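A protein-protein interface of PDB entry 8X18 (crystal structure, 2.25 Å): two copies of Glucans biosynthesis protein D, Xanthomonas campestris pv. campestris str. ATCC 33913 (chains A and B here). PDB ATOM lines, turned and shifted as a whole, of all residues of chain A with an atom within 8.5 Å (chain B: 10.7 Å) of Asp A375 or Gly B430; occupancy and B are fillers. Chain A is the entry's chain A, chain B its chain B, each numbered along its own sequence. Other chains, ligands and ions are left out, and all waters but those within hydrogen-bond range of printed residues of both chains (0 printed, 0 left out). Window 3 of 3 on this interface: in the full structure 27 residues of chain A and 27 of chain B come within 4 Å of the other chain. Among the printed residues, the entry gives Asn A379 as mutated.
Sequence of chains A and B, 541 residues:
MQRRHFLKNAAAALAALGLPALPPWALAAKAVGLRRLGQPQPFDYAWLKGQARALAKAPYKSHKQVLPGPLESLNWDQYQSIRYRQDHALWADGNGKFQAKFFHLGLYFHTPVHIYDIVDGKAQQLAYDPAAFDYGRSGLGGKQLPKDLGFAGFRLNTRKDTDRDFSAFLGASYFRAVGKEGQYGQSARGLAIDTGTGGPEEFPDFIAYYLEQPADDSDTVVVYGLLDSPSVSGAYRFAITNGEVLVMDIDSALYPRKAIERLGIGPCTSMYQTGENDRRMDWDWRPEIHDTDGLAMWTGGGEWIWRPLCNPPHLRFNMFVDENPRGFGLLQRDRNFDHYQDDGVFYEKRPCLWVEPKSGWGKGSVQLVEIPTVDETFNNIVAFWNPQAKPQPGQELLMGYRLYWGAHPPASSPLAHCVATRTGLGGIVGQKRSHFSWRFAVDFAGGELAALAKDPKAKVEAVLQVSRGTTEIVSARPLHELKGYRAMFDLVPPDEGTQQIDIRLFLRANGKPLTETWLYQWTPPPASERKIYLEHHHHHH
The backbone carbonyl oxygen (O) of Trp A283 lies within hydrogen-bond range of the backbone NH (N) of Leu B425 (2.7 Å).
The side-chain hydroxyl (OH) of Tyr A347 lies within hydrogen-bond range of the side-chain carboxylate (OE2) of Glu A376 (2.6 Å). NH2 of Arg A286 lies within salt-bridge range of OE1 of Glu A376 (2.8 Å). The side-chain hydroxyl (OG1) of Thr A373 lies within hydrogen-bond range of the backbone carbonyl oxygen (O) of Asp A375 (2.7 Å). The side-chain amide oxygen (OE1) of Gln A273 lies within hydrogen-bond range of the backbone NH (N) of Glu A376, 3.2 Å away. The side-chain carboxylate of Asp A375 sits at hydrogen-bond distance from the side-chain hydroxyl of Thr A377 (2.6 Å).
Among the printed residues, merely in contact across the chains: Trp A283 with Ile B532, Asp A375 with Gly B430 and Glu A376 with Val B429.
Asp A375 touches just one residue of chain B: Gly B430 (3.5 Å). Printed residues of chain A within 4 Å of Ile B532: Trp A283 (3.7 Å). Of the printed residues of chain A, Val B429 touches Glu A376 (3.3 Å). Of the printed residues of chain B, Trp A283 touches Leu B425 and Ile B532. Printed residues of chain A within 4 Å of Leu B425: Trp A283. Arg A280 touches none of the printed residues of chain B. The nearest printed residue of chain B that does not touch Asp A375 is Val B429 (5.3 Å). The nearest residue of chain A that does not touch Gly B430 is Thr A377 (4.05 Å).
Of the 14 printed residues of chain B, 4 touch a printed residue of chain A. Printed residues of chain B that touch a printed residue of chain A: Leu B425, Val B429, Gly B430 and Ile B532. Of the 22 printed residues of chain A, 3 touch a printed residue of chain B. Among the printed residues, 4 pairs touch across the chains. Among the printed residues, no Asp or Glu carboxylate lies within 4 Å of a Lys or Arg side-chain nitrogen of the other chain.
No position is printed for both chains. Of the 4 pairs that touch across the chains among the printed residues, none has its exchanged pair printed and touching as well.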
ATOM      1  N   MET A 271       3.792   3.903  -7.755  1.00  0.00           N
ATOM      2  CA  MET A 271       5.022   4.231  -8.481  1.00  0.00           C
ATOM      3  C   MET A 271       6.191   3.482  -7.826  1.00  0.00           C
ATOM      4  O   MET A 271       6.295   3.390  -6.592  1.00  0.00           O
ATOM      5  CB  MET A 271       5.265   5.745  -8.440  1.00  0.00           C
ATOM      6  CG  MET A 271       6.577   6.213  -9.088  1.00  0.00           C
ATOM      7  SD  MET A 271       8.029   6.089  -8.014  1.00  0.00           S
ATOM      8  CE  MET A 271       7.572   7.299  -6.756  1.00  0.00           C
ATOM      9  N   TYR A 272       7.000   2.842  -8.666  1.00  0.00           N
ATOM     10  CA  TYR A 272       8.238   2.235  -8.243  1.00  0.00           C
ATOM     11  C   TYR A 272       9.331   2.613  -9.245  1.00  0.00           C
ATOM     12  O   TYR A 272       9.376   2.069 -10.355  1.00  0.00           O
ATOM     13  CB  TYR A 272       8.080   0.707  -8.110  1.00  0.00           C
ATOM     14  CG  TYR A 272       9.292   0.073  -7.473  1.00  0.00           C
ATOM     15  CD1 TYR A 272      10.453  -0.154  -8.190  1.00  0.00           C
ATOM     16  CD2 TYR A 272       9.333  -0.170  -6.115  1.00  0.00           C
ATOM     17  CE1 TYR A 272      11.599  -0.660  -7.589  1.00  0.00           C
ATOM     18  CE2 TYR A 272      10.461  -0.691  -5.499  1.00  0.00           C
ATOM     19  CZ  TYR A 272      11.602  -0.944  -6.239  1.00  0.00           C
ATOM     20  OH  TYR A 272      12.711  -1.436  -5.602  1.00  0.00           O
ATOM     21  N   GLN A 273      10.264   3.496  -8.852  1.00  0.00           N
ATOM     22  CA  GLN A 273      11.365   3.803  -9.753  1.00  0.00           C
ATOM     23  C   GLN A 273      12.557   2.887  -9.491  1.00  0.00           C
ATOM     24  O   GLN A 273      13.167   2.352 -10.429  1.00  0.00           O
ATOM     25  CB  GLN A 273      11.804   5.262  -9.651  1.00  0.00           C
ATOM     26  CG  GLN A 273      12.957   5.604 -10.615  1.00  0.00           C
ATOM     27  CD  GLN A 273      13.496   6.992 -10.397  1.00  0.00           C
ATOM     28  OE1 GLN A 273      12.757   7.933 -10.128  1.00  0.00           O
ATOM     29  NE2 GLN A 273      14.807   7.130 -10.471  1.00  0.00           N
ATOM     30  N   THR A 274      12.997   2.827  -8.243  1.00  0.00           N
ATOM     31  CA  THR A 274      14.242   2.119  -7.954  1.00  0.00           C
ATOM     32  C   THR A 274      14.273   1.777  -6.478  1.00  0.00           C
ATOM     33  O   THR A 274      13.599   2.402  -5.657  1.00  0.00           O
ATOM     34  CB  THR A 274      15.477   2.965  -8.307  1.00  0.00           C
ATOM     35  OG1 THR A 274      16.649   2.164  -8.259  1.00  0.00           O
ATOM     36  CG2 THR A 274      15.660   4.155  -7.388  1.00  0.00           C
ATOM     37  N   ARG A 280      17.696  -1.367 -11.682  1.00  0.00           N
ATOM     38  CA  ARG A 280      17.876  -1.019 -13.091  1.00  0.00           C
ATOM     39  C   ARG A 280      17.947   0.495 -13.301  1.00  0.00           C
ATOM     40  O   ARG A 280      18.801   0.962 -14.041  1.00  0.00           O
ATOM     41  CB  ARG A 280      16.714  -1.567 -13.932  1.00  0.00           C
ATOM     42  CG  ARG A 280      16.949  -1.566 -15.437  1.00  0.00           C
ATOM     43  CD  ARG A 280      15.759  -2.092 -16.264  1.00  0.00           C
ATOM     44  NE  ARG A 280      14.526  -1.299 -16.126  1.00  0.00           N
ATOM     45  CZ  ARG A 280      14.259  -0.128 -16.710  1.00  0.00           C
ATOM     46  NH1 ARG A 280      15.077   0.361 -17.618  1.00  0.00           N
ATOM     47  NH2 ARG A 280      13.147   0.547 -16.429  1.00  0.00           N
ATOM     48  N   MET A 281      17.019   1.235 -12.714  1.00  0.00           N
ATOM     49  CA  MET A 281      17.018   2.709 -12.837  1.00  0.00           C
ATOM     50  C   MET A 281      17.570   3.340 -11.552  1.00  0.00           C
ATOM     51  O   MET A 281      16.866   4.161 -10.961  1.00  0.00           O
ATOM     52  CB  MET A 281      15.609   3.224 -13.141  1.00  0.00           C
ATOM     53  CG  MET A 281      15.224   3.096 -14.598  1.00  0.00           C
ATOM     54  SD  MET A 281      16.150   4.221 -15.665  1.00  0.00           S
ATOM     55  CE  MET A 281      16.968   3.046 -16.738  1.00  0.00           C
ATOM     56  N   TRP A 283      19.618   5.852 -10.983  1.00  0.00           N
ATOM     57  CA  TRP A 283      20.283   7.080 -11.484  1.00  0.00           C
ATOM     58  C   TRP A 283      20.230   8.191 -10.442  1.00  0.00           C
ATOM     59  O   TRP A 283      20.770   9.251 -10.714  1.00  0.00           O
ATOM     60  CB  TRP A 283      19.543   7.553 -12.736  1.00  0.00           C
ATOM     61  CG  TRP A 283      19.679   6.725 -13.972  1.00  0.00           C
ATOM     62  CD1 TRP A 283      20.337   5.541 -14.124  1.00  0.00           C
ATOM     63  CD2 TRP A 283      19.122   7.045 -15.256  1.00  0.00           C
ATOM     64  NE1 TRP A 283      20.231   5.108 -15.417  1.00  0.00           N
ATOM     65  CE2 TRP A 283      19.492   6.009 -16.134  1.00  0.00           C
ATOM     66  CE3 TRP A 283      18.356   8.106 -15.745  1.00  0.00           C
ATOM     67  CZ2 TRP A 283      19.115   6.007 -17.474  1.00  0.00           C
ATOM     68  CZ3 TRP A 283      17.986   8.103 -17.071  1.00  0.00           C
ATOM     69  CH2 TRP A 283      18.362   7.066 -17.920  1.00  0.00           C
ATOM     70  N   ASP A 284      19.602   7.952  -9.303  1.00  0.00           N
ATOM     71  CA  ASP A 284      19.369   9.017  -8.354  1.00  0.00           C
ATOM     72  C   ASP A 284      20.336   8.864  -7.185  1.00  0.00           C
ATOM     73  O   ASP A 284      20.816   7.764  -6.923  1.00  0.00           O
ATOM     74  CB  ASP A 284      17.911   8.999  -7.879  1.00  0.00           C
ATOM     75  CG  ASP A 284      17.399  10.344  -7.405  1.00  0.00           C
ATOM     76  OD1 ASP A 284      17.714  10.720  -6.249  1.00  0.00           O
ATOM     77  OD2 ASP A 284      16.729  11.019  -8.213  1.00  0.00           O
ATOM     78  N   ARG A 286      19.191   9.352  -4.211  1.00  0.00           N
ATOM     79  CA  ARG A 286      18.294   8.663  -3.289  1.00  0.00           C
ATOM     80  C   ARG A 286      18.240   7.186  -3.647  1.00  0.00           C
ATOM     81  O   ARG A 286      17.980   6.849  -4.796  1.00  0.00           O
ATOM     82  CB  ARG A 286      16.876   9.236  -3.306  1.00  0.00           C
ATOM     83  CG  ARG A 286      16.851  10.667  -2.778  1.00  0.00           C
ATOM     84  CD  ARG A 286      15.612  11.447  -3.154  1.00  0.00           C
ATOM     85  NE  ARG A 286      15.566  11.574  -4.599  1.00  0.00           N
ATOM     86  CZ  ARG A 286      14.445  11.718  -5.295  1.00  0.00           C
ATOM     87  NH1 ARG A 286      13.279  11.832  -4.673  1.00  0.00           N
ATOM     88  NH2 ARG A 286      14.523  11.751  -6.607  1.00  0.00           N
ATOM     89  N   ILE A 289      13.208   4.926  -4.218  1.00  0.00           N
ATOM     90  CA  ILE A 289      12.228   5.857  -4.740  1.00  0.00           C
ATOM     91  C   ILE A 289      11.030   5.040  -5.191  1.00  0.00           C
ATOM     92  O   ILE A 289      11.058   4.406  -6.251  1.00  0.00           O
ATOM     93  CB  ILE A 289      12.805   6.715  -5.884  1.00  0.00           C
ATOM     94  CG1 ILE A 289      14.034   7.535  -5.468  1.00  0.00           C
ATOM     95  CG2 ILE A 289      11.730   7.628  -6.412  1.00  0.00           C
ATOM     96  CD1 ILE A 289      14.723   8.254  -6.599  1.00  0.00           C
ATOM     97  N   ASN A 311      10.795  -2.172 -11.637  1.00  0.00           N
ATOM     98  CA  ASN A 311      10.699  -1.172 -12.685  1.00  0.00           C
ATOM     99  C   ASN A 311      11.330  -1.785 -13.930  1.00  0.00           C
ATOM    100  O   ASN A 311      12.481  -1.548 -14.237  1.00  0.00           O
ATOM    101  CB  ASN A 311      11.357   0.144 -12.291  1.00  0.00           C
ATOM    102  CG  ASN A 311      11.341   1.193 -13.393  1.00  0.00           C
ATOM    103  OD1 ASN A 311      10.688   1.060 -14.441  1.00  0.00           O
ATOM    104  ND2 ASN A 311      12.027   2.289 -13.134  1.00  0.00           N
ATOM    105  N   TYR A 347       8.826   9.521   1.485  1.00  0.00           N
ATOM    106  CA  TYR A 347       8.351   8.266   0.909  1.00  0.00           C
ATOM    107  C   TYR A 347       8.015   7.216   1.978  1.00  0.00           C
ATOM    108  O   TYR A 347       7.045   6.451   1.824  1.00  0.00           O
ATOM    109  CB  TYR A 347       9.378   7.735  -0.093  1.00  0.00           C
ATOM    110  CG  TYR A 347       9.343   8.400  -1.439  1.00  0.00           C
ATOM    111  CD1 TYR A 347       8.215   8.311  -2.242  1.00  0.00           C
ATOM    112  CD2 TYR A 347      10.439   9.097  -1.941  1.00  0.00           C
ATOM    113  CE1 TYR A 347       8.183   8.860  -3.521  1.00  0.00           C
ATOM    114  CE2 TYR A 347      10.414   9.669  -3.210  1.00  0.00           C
ATOM    115  CZ  TYR A 347       9.272   9.586  -3.990  1.00  0.00           C
ATOM    116  OH  TYR A 347       9.196  10.151  -5.232  1.00  0.00           O
ATOM    117  N   ILE A 371       4.926  -0.754 -15.599  1.00  0.00           N
ATOM    118  CA  ILE A 371       5.349   0.013 -16.770  1.00  0.00           C
ATOM    119  C   ILE A 371       6.767   0.557 -16.545  1.00  0.00           C
ATOM    120  O   ILE A 371       7.090   1.008 -15.446  1.00  0.00           O
ATOM    121  CB  ILE A 371       4.323   1.139 -17.033  1.00  0.00           C
ATOM    122  CG1 ILE A 371       2.892   0.598 -16.999  1.00  0.00           C
ATOM    123  CG2 ILE A 371       4.618   1.923 -18.341  1.00  0.00           C
ATOM    124  CD1 ILE A 371       1.803   1.687 -16.974  1.00  0.00           C
ATOM    125  N   PRO A 372       7.680   0.552 -17.540  1.00  0.00           N
ATOM    126  CA  PRO A 372       9.001   1.173 -17.370  1.00  0.00           C
ATOM    127  C   PRO A 372       8.844   2.639 -17.011  1.00  0.00           C
ATOM    128  O   PRO A 372       7.985   3.303 -17.555  1.00  0.00           O
ATOM    129  CB  PRO A 372       9.679   1.105 -18.765  1.00  0.00           C
ATOM    130  CG  PRO A 372       8.918  -0.024 -19.491  1.00  0.00           C
ATOM    131  CD  PRO A 372       7.513  -0.013 -18.889  1.00  0.00           C
ATOM    132  N   THR A 373       9.646   3.155 -16.102  1.00  0.00           N
ATOM    133  CA  THR A 373       9.637   4.591 -15.887  1.00  0.00           C
ATOM    134  C   THR A 373      11.060   5.074 -15.688  1.00  0.00           C
ATOM    135  O   THR A 373      11.896   4.350 -15.120  1.00  0.00           O
ATOM    136  CB  THR A 373       8.779   4.946 -14.670  1.00  0.00           C
ATOM    137  OG1 THR A 373       8.570   6.357 -14.641  1.00  0.00           O
ATOM    138  CG2 THR A 373       9.413   4.514 -13.356  1.00  0.00           C
ATOM    139  N   VAL A 374      11.316   6.305 -16.133  1.00  0.00           N
ATOM    140  CA  VAL A 374      12.644   6.897 -15.973  1.00  0.00           C
ATOM    141  C   VAL A 374      12.600   7.815 -14.782  1.00  0.00           C
ATOM    142  O   VAL A 374      13.640   8.234 -14.353  1.00  0.00           O
ATOM    143  CB  VAL A 374      13.157   7.691 -17.195  1.00  0.00           C
ATOM    144  CG1 VAL A 374      13.225   6.803 -18.429  1.00  0.00           C
ATOM    145  CG2 VAL A 374      12.304   8.922 -17.486  1.00  0.00           C
ATOM    146  N   ASP A 375      11.418   8.168 -14.283  1.00  0.00           N
ATOM    147  CA  ASP A 375      11.400   8.999 -13.097  1.00  0.00           C
ATOM    148  C   ASP A 375      10.123   8.767 -12.262  1.00  0.00           C
ATOM    149  O   ASP A 375       9.234   7.980 -12.618  1.00  0.00           O
ATOM    150  CB  ASP A 375      11.675  10.436 -13.544  1.00  0.00           C
ATOM    151  CG  ASP A 375      10.485  11.082 -14.246  1.00  0.00           C
ATOM    152  OD1 ASP A 375       9.345  10.608 -14.017  1.00  0.00           O
ATOM    153  OD2 ASP A 375      10.705  12.066 -15.015  1.00  0.00           O
ATOM    154  N   GLU A 376      10.075   9.458 -11.113  1.00  0.00           N
ATOM    155  CA  GLU A 376       9.048   9.213 -10.065  1.00  0.00           C
ATOM    156  C   GLU A 376       7.749   9.991 -10.251  1.00  0.00           C
ATOM    157  O   GLU A 376       6.908   9.914  -9.357  1.00  0.00           O
ATOM    158  CB  GLU A 376       9.689   9.613  -8.734  1.00  0.00           C
ATOM    159  CG  GLU A 376       9.917  11.107  -8.572  1.00  0.00           C
ATOM    160  CD  GLU A 376      11.063  11.506  -7.655  1.00  0.00           C
ATOM    161  OE1 GLU A 376      12.195  11.606  -8.139  1.00  0.00           O
ATOM    162  OE2 GLU A 376      10.818  11.728  -6.462  1.00  0.00           O
ATOM    163  N   THR A 377       7.604  10.679 -11.366  1.00  0.00           N
ATOM    164  CA  THR A 377       6.429  11.512 -11.624  1.00  0.00           C
ATOM    165  C   THR A 377       5.298  10.717 -12.275  1.00  0.00           C
ATOM    166  O   THR A 377       4.186  11.172 -12.325  1.00  0.00           O
ATOM    167  CB  THR A 377       6.775  12.721 -12.521  1.00  0.00           C
ATOM    168  OG1 THR A 377       7.398  12.371 -13.764  1.00  0.00           O
ATOM    169  CG2 THR A 377       7.752  13.639 -11.823  1.00  0.00           C
ATOM    170  N   PHE A 378       5.562   9.503 -12.721  1.00  0.00           N
ATOM    171  CA  PHE A 378       4.568   8.705 -13.400  1.00  0.00           C
ATOM    172  C   PHE A 378       4.206   7.498 -12.498  1.00  0.00           C
ATOM    173  O   PHE A 378       5.078   6.850 -11.930  1.00  0.00           O
ATOM    174  CB  PHE A 378       5.173   8.393 -14.773  1.00  0.00           C
ATOM    175  CG  PHE A 378       4.494   7.283 -15.527  1.00  0.00           C
ATOM    176  CD1 PHE A 378       3.201   7.433 -15.995  1.00  0.00           C
ATOM    177  CD2 PHE A 378       5.148   6.099 -15.777  1.00  0.00           C
ATOM    178  CE1 PHE A 378       2.580   6.409 -16.692  1.00  0.00           C
ATOM    179  CE2 PHE A 378       4.523   5.081 -16.465  1.00  0.00           C
ATOM    180  CZ  PHE A 378       3.239   5.227 -16.905  1.00  0.00           C
ATOM    181  N   ASN A 379       2.917   7.201 -12.406  1.00  0.00           N
ATOM    182  CA  ASN A 379       2.449   6.021 -11.633  1.00  0.00           C
ATOM    183  C   ASN A 379       2.592   4.769 -12.509  1.00  0.00           C
ATOM    184  O   ASN A 379       1.668   4.469 -13.255  1.00  0.00           O
ATOM    185  CB  ASN A 379       1.044   6.278 -11.102  1.00  0.00           C
ATOM    186  CG  ASN A 379       1.014   7.343 -10.030  1.00  0.00           C
ATOM    187  OD1 ASN A 379       0.166   8.229 -10.058  1.00  0.00           O
ATOM    188  ND2 ASN A 379       1.938   7.269  -9.088  1.00  0.00           N
ATOM    189  N   ASN A 380       3.697   4.047 -12.366  1.00  0.00           N
ATOM    190  CA  ASN A 380       3.974   2.948 -13.266  1.00  0.00           C
ATOM    191  C   ASN A 380       3.529   1.592 -12.693  1.00  0.00           C
ATOM    192  O   ASN A 380       3.862   0.556 -13.300  1.00  0.00           O
ATOM    193  CB  ASN A 380       5.459   2.953 -13.607  1.00  0.00           C
ATOM    194  CG  ASN A 380       6.345   2.716 -12.395  1.00  0.00           C
ATOM    195  OD1 ASN A 380       6.093   3.220 -11.307  1.00  0.00           O
ATOM    196  ND2 ASN A 380       7.343   1.879 -12.559  1.00  0.00           N
ATOM    197  N   LEU B 425      22.156  11.551 -11.148  1.00  0.00           N
ATOM    198  CA  LEU B 425      21.835  12.427 -12.268  1.00  0.00           C
ATOM    199  C   LEU B 425      21.241  13.748 -11.756  1.00  0.00           C
ATOM    200  O   LEU B 425      20.362  13.771 -10.896  1.00  0.00           O
ATOM    201  CB  LEU B 425      20.902  11.712 -13.258  1.00  0.00           C
ATOM    202  CG  LEU B 425      20.605  12.498 -14.545  1.00  0.00           C
ATOM    203  CD1 LEU B 425      21.884  12.661 -15.352  1.00  0.00           C
ATOM    204  CD2 LEU B 425      19.523  11.831 -15.392  1.00  0.00           C
ATOM    205  N   GLY B 426      21.785  14.862 -12.256  1.00  0.00           N
ATOM    206  CA  GLY B 426      21.339  16.189 -11.856  1.00  0.00           C
ATOM    207  C   GLY B 426      20.127  16.673 -12.647  1.00  0.00           C
ATOM    208  O   GLY B 426      19.656  16.009 -13.562  1.00  0.00           O
ATOM    209  N   GLY B 427      19.625  17.842 -12.273  1.00  0.00           N
ATOM    210  CA  GLY B 427      18.464  18.409 -12.929  1.00  0.00           C
ATOM    211  C   GLY B 427      17.225  18.317 -12.050  1.00  0.00           C
ATOM    212  O   GLY B 427      17.079  17.385 -11.261  1.00  0.00           O
ATOM    213  N   ILE B 428      16.357  19.324 -12.168  1.00  0.00           N
ATOM    214  CA  ILE B 428      15.085  19.323 -11.474  1.00  0.00           C
ATOM    215  C   ILE B 428      14.292  18.102 -11.948  1.00  0.00           C
ATOM    216  O   ILE B 428      14.166  17.835 -13.148  1.00  0.00           O
ATOM    217  CB  ILE B 428      14.338  20.660 -11.660  1.00  0.00           C
ATOM    218  CG1 ILE B 428      15.093  21.814 -10.992  1.00  0.00           C
ATOM    219  CG2 ILE B 428      12.910  20.557 -11.128  1.00  0.00           C
ATOM    220  CD1 ILE B 428      14.481  23.184 -11.232  1.00  0.00           C
ATOM    221  N   VAL B 429      13.843  17.318 -10.969  1.00  0.00           N
ATOM    222  CA  VAL B 429      13.200  16.035 -11.202  1.00  0.00           C
ATOM    223  C   VAL B 429      11.936  16.224 -12.043  1.00  0.00           C
ATOM    224  O   VAL B 429      11.081  17.023 -11.694  1.00  0.00           O
ATOM    225  CB  VAL B 429      12.890  15.347  -9.857  1.00  0.00           C
ATOM    226  CG1 VAL B 429      11.792  14.303  -9.975  1.00  0.00           C
ATOM    227  CG2 VAL B 429      14.154  14.745  -9.273  1.00  0.00           C
ATOM    228  N   GLY B 430      11.841  15.452 -13.132  1.00  0.00           N
ATOM    229  CA  GLY B 430      10.663  15.439 -13.983  1.00  0.00           C
ATOM    230  C   GLY B 430      10.569  16.662 -14.897  1.00  0.00           C
ATOM    231  O   GLY B 430       9.470  17.077 -15.230  1.00  0.00           O
ATOM    232  N   GLN B 431      11.716  17.241 -15.280  1.00  0.00           N
ATOM    233  CA  GLN B 431      11.765  18.342 -16.230  1.00  0.00           C
ATOM    234  C   GLN B 431      12.677  17.951 -17.382  1.00  0.00           C
ATOM    235  O   GLN B 431      13.615  17.194 -17.197  1.00  0.00           O
ATOM    236  CB  GLN B 431      12.308  19.623 -15.602  1.00  0.00           C
ATOM    237  CG  GLN B 431      11.269  20.421 -14.829  1.00  0.00           C
ATOM    238  CD  GLN B 431      11.723  21.843 -14.568  1.00  0.00           C
ATOM    239  OE1 GLN B 431      12.607  22.382 -15.245  1.00  0.00           O
ATOM    240  NE2 GLN B 431      11.108  22.467 -13.574  1.00  0.00           N
ATOM    241  N   LYS B 432      12.417  18.495 -18.564  1.00  0.00           N
ATOM    242  CA  LYS B 432      13.322  18.297 -19.680  1.00  0.00           C
ATOM    243  C   LYS B 432      14.660  18.955 -19.317  1.00  0.00           C
ATOM    244  O   LYS B 432      14.710  20.029 -18.704  1.00  0.00           O
ATOM    245  CB  LYS B 432      12.649  18.826 -20.956  1.00  0.00           C
ATOM    246  CG  LYS B 432      12.942  18.062 -22.249  1.00  0.00           C
ATOM    247  CD  LYS B 432      13.895  18.759 -23.220  1.00  0.00           C
ATOM    248  CE  LYS B 432      13.935  18.079 -24.574  1.00  0.00           C
ATOM    249  NZ  LYS B 432      14.317  16.647 -24.466  1.00  0.00           N
ATOM    250  N   ARG B 433      15.754  18.268 -19.654  1.00  0.00           N
ATOM    251  CA  ARG B 433      17.091  18.754 -19.357  1.00  0.00           C
ATOM    252  C   ARG B 433      17.708  19.319 -20.621  1.00  0.00           C
ATOM    253  O   ARG B 433      17.813  18.587 -21.596  1.00  0.00           O
ATOM    254  CB  ARG B 433      18.012  17.608 -18.939  1.00  0.00           C
ATOM    255  CG  ARG B 433      17.720  17.021 -17.574  1.00  0.00           C
ATOM    256  CD  ARG B 433      18.329  15.632 -17.505  1.00  0.00           C
ATOM    257  NE  ARG B 433      18.246  15.021 -16.188  1.00  0.00           N
ATOM    258  CZ  ARG B 433      17.186  15.053 -15.381  1.00  0.00           C
ATOM    259  NH1 ARG B 433      16.169  15.862 -15.603  1.00  0.00           N
ATOM    260  NH2 ARG B 433      17.170  14.318 -14.291  1.00  0.00           N
ATOM    261  N   SER B 434      18.151  20.582 -20.577  1.00  0.00           N
ATOM    262  CA  SER B 434      18.870  21.164 -21.702  1.00  0.00           C
ATOM    263  C   SER B 434      20.317  20.682 -21.677  1.00  0.00           C
ATOM    264  O   SER B 434      20.959  20.645 -22.723  1.00  0.00           O
ATOM    265  CB  SER B 434      18.757  22.697 -21.771  1.00  0.00           C
ATOM    266  OG  SER B 434      19.221  23.354 -20.594  1.00  0.00           O
ATOM    267  N   ARG B 439      24.306  15.524  -9.699  1.00  0.00           N
ATOM    268  CA  ARG B 439      23.846  15.998  -8.408  1.00  0.00           C
ATOM    269  C   ARG B 439      24.590  15.293  -7.262  1.00  0.00           C
ATOM    270  O   ARG B 439      24.743  14.080  -7.262  1.00  0.00           O
ATOM    271  CB  ARG B 439      22.349  15.711  -8.306  1.00  0.00           C
ATOM    272  CG  ARG B 439      21.731  16.159  -6.991  1.00  0.00           C
ATOM    273  CD  ARG B 439      20.230  16.425  -7.061  1.00  0.00           C
ATOM    274  NE  ARG B 439      19.945  17.477  -8.004  1.00  0.00           N
ATOM    275  CZ  ARG B 439      18.777  18.097  -8.158  1.00  0.00           C
ATOM    276  NH1 ARG B 439      17.676  17.670  -7.563  1.00  0.00           N
ATOM    277  NH2 ARG B 439      18.708  19.132  -8.978  1.00  0.00           N
ATOM    278  N   ILE B 473      21.976  25.201  -8.508  1.00  0.00           N
ATOM    279  CA  ILE B 473      20.972  24.637  -7.612  1.00  0.00           C
ATOM    280  C   ILE B 473      21.646  24.185  -6.309  1.00  0.00           C
ATOM    281  O   ILE B 473      21.521  23.026  -5.899  1.00  0.00           O
ATOM    282  CB  ILE B 473      20.180  23.491  -8.289  1.00  0.00           C
ATOM    283  CG1 ILE B 473      19.777  23.864  -9.730  1.00  0.00           C
ATOM    284  CG2 ILE B 473      18.971  23.118  -7.418  1.00  0.00           C
ATOM    285  CD1 ILE B 473      19.045  22.778 -10.510  1.00  0.00           C
ATOM    286  N   ASP B 490      24.319  20.782  -8.037  1.00  0.00           N
ATOM    287  CA  ASP B 490      24.562  20.127  -9.312  1.00  0.00           C
ATOM    288  C   ASP B 490      25.818  20.707  -9.986  1.00  0.00           C
ATOM    289  O   ASP B 490      26.095  21.903  -9.916  1.00  0.00           O
ATOM    290  CB  ASP B 490      23.366  20.286 -10.245  1.00  0.00           C
ATOM    291  CG  ASP B 490      22.066  19.625  -9.807  1.00  0.00           C
ATOM    292  OD1 ASP B 490      22.023  19.028  -8.688  1.00  0.00           O
ATOM    293  OD2 ASP B 490      21.063  19.767 -10.582  1.00  0.00           O
ATOM    294  N   ILE B 532      22.420   8.602 -23.044  1.00  0.00           N
ATOM    295  CA  ILE B 532      21.438   7.734 -22.410  1.00  0.00           C
ATOM    296  C   ILE B 532      20.695   8.477 -21.300  1.00  0.00           C
ATOM    297  O   ILE B 532      19.477   8.406 -21.229  1.00  0.00           O
ATOM    298  CB  ILE B 532      22.112   6.459 -21.899  1.00  0.00           C
ATOM    299  CG1 ILE B 532      22.627   5.610 -23.070  1.00  0.00           C
ATOM    300  CG2 ILE B 532      21.171   5.705 -20.982  1.00  0.00           C
ATOM    301  CD1 ILE B 532      23.706   4.616 -22.676  1.00  0.00           C
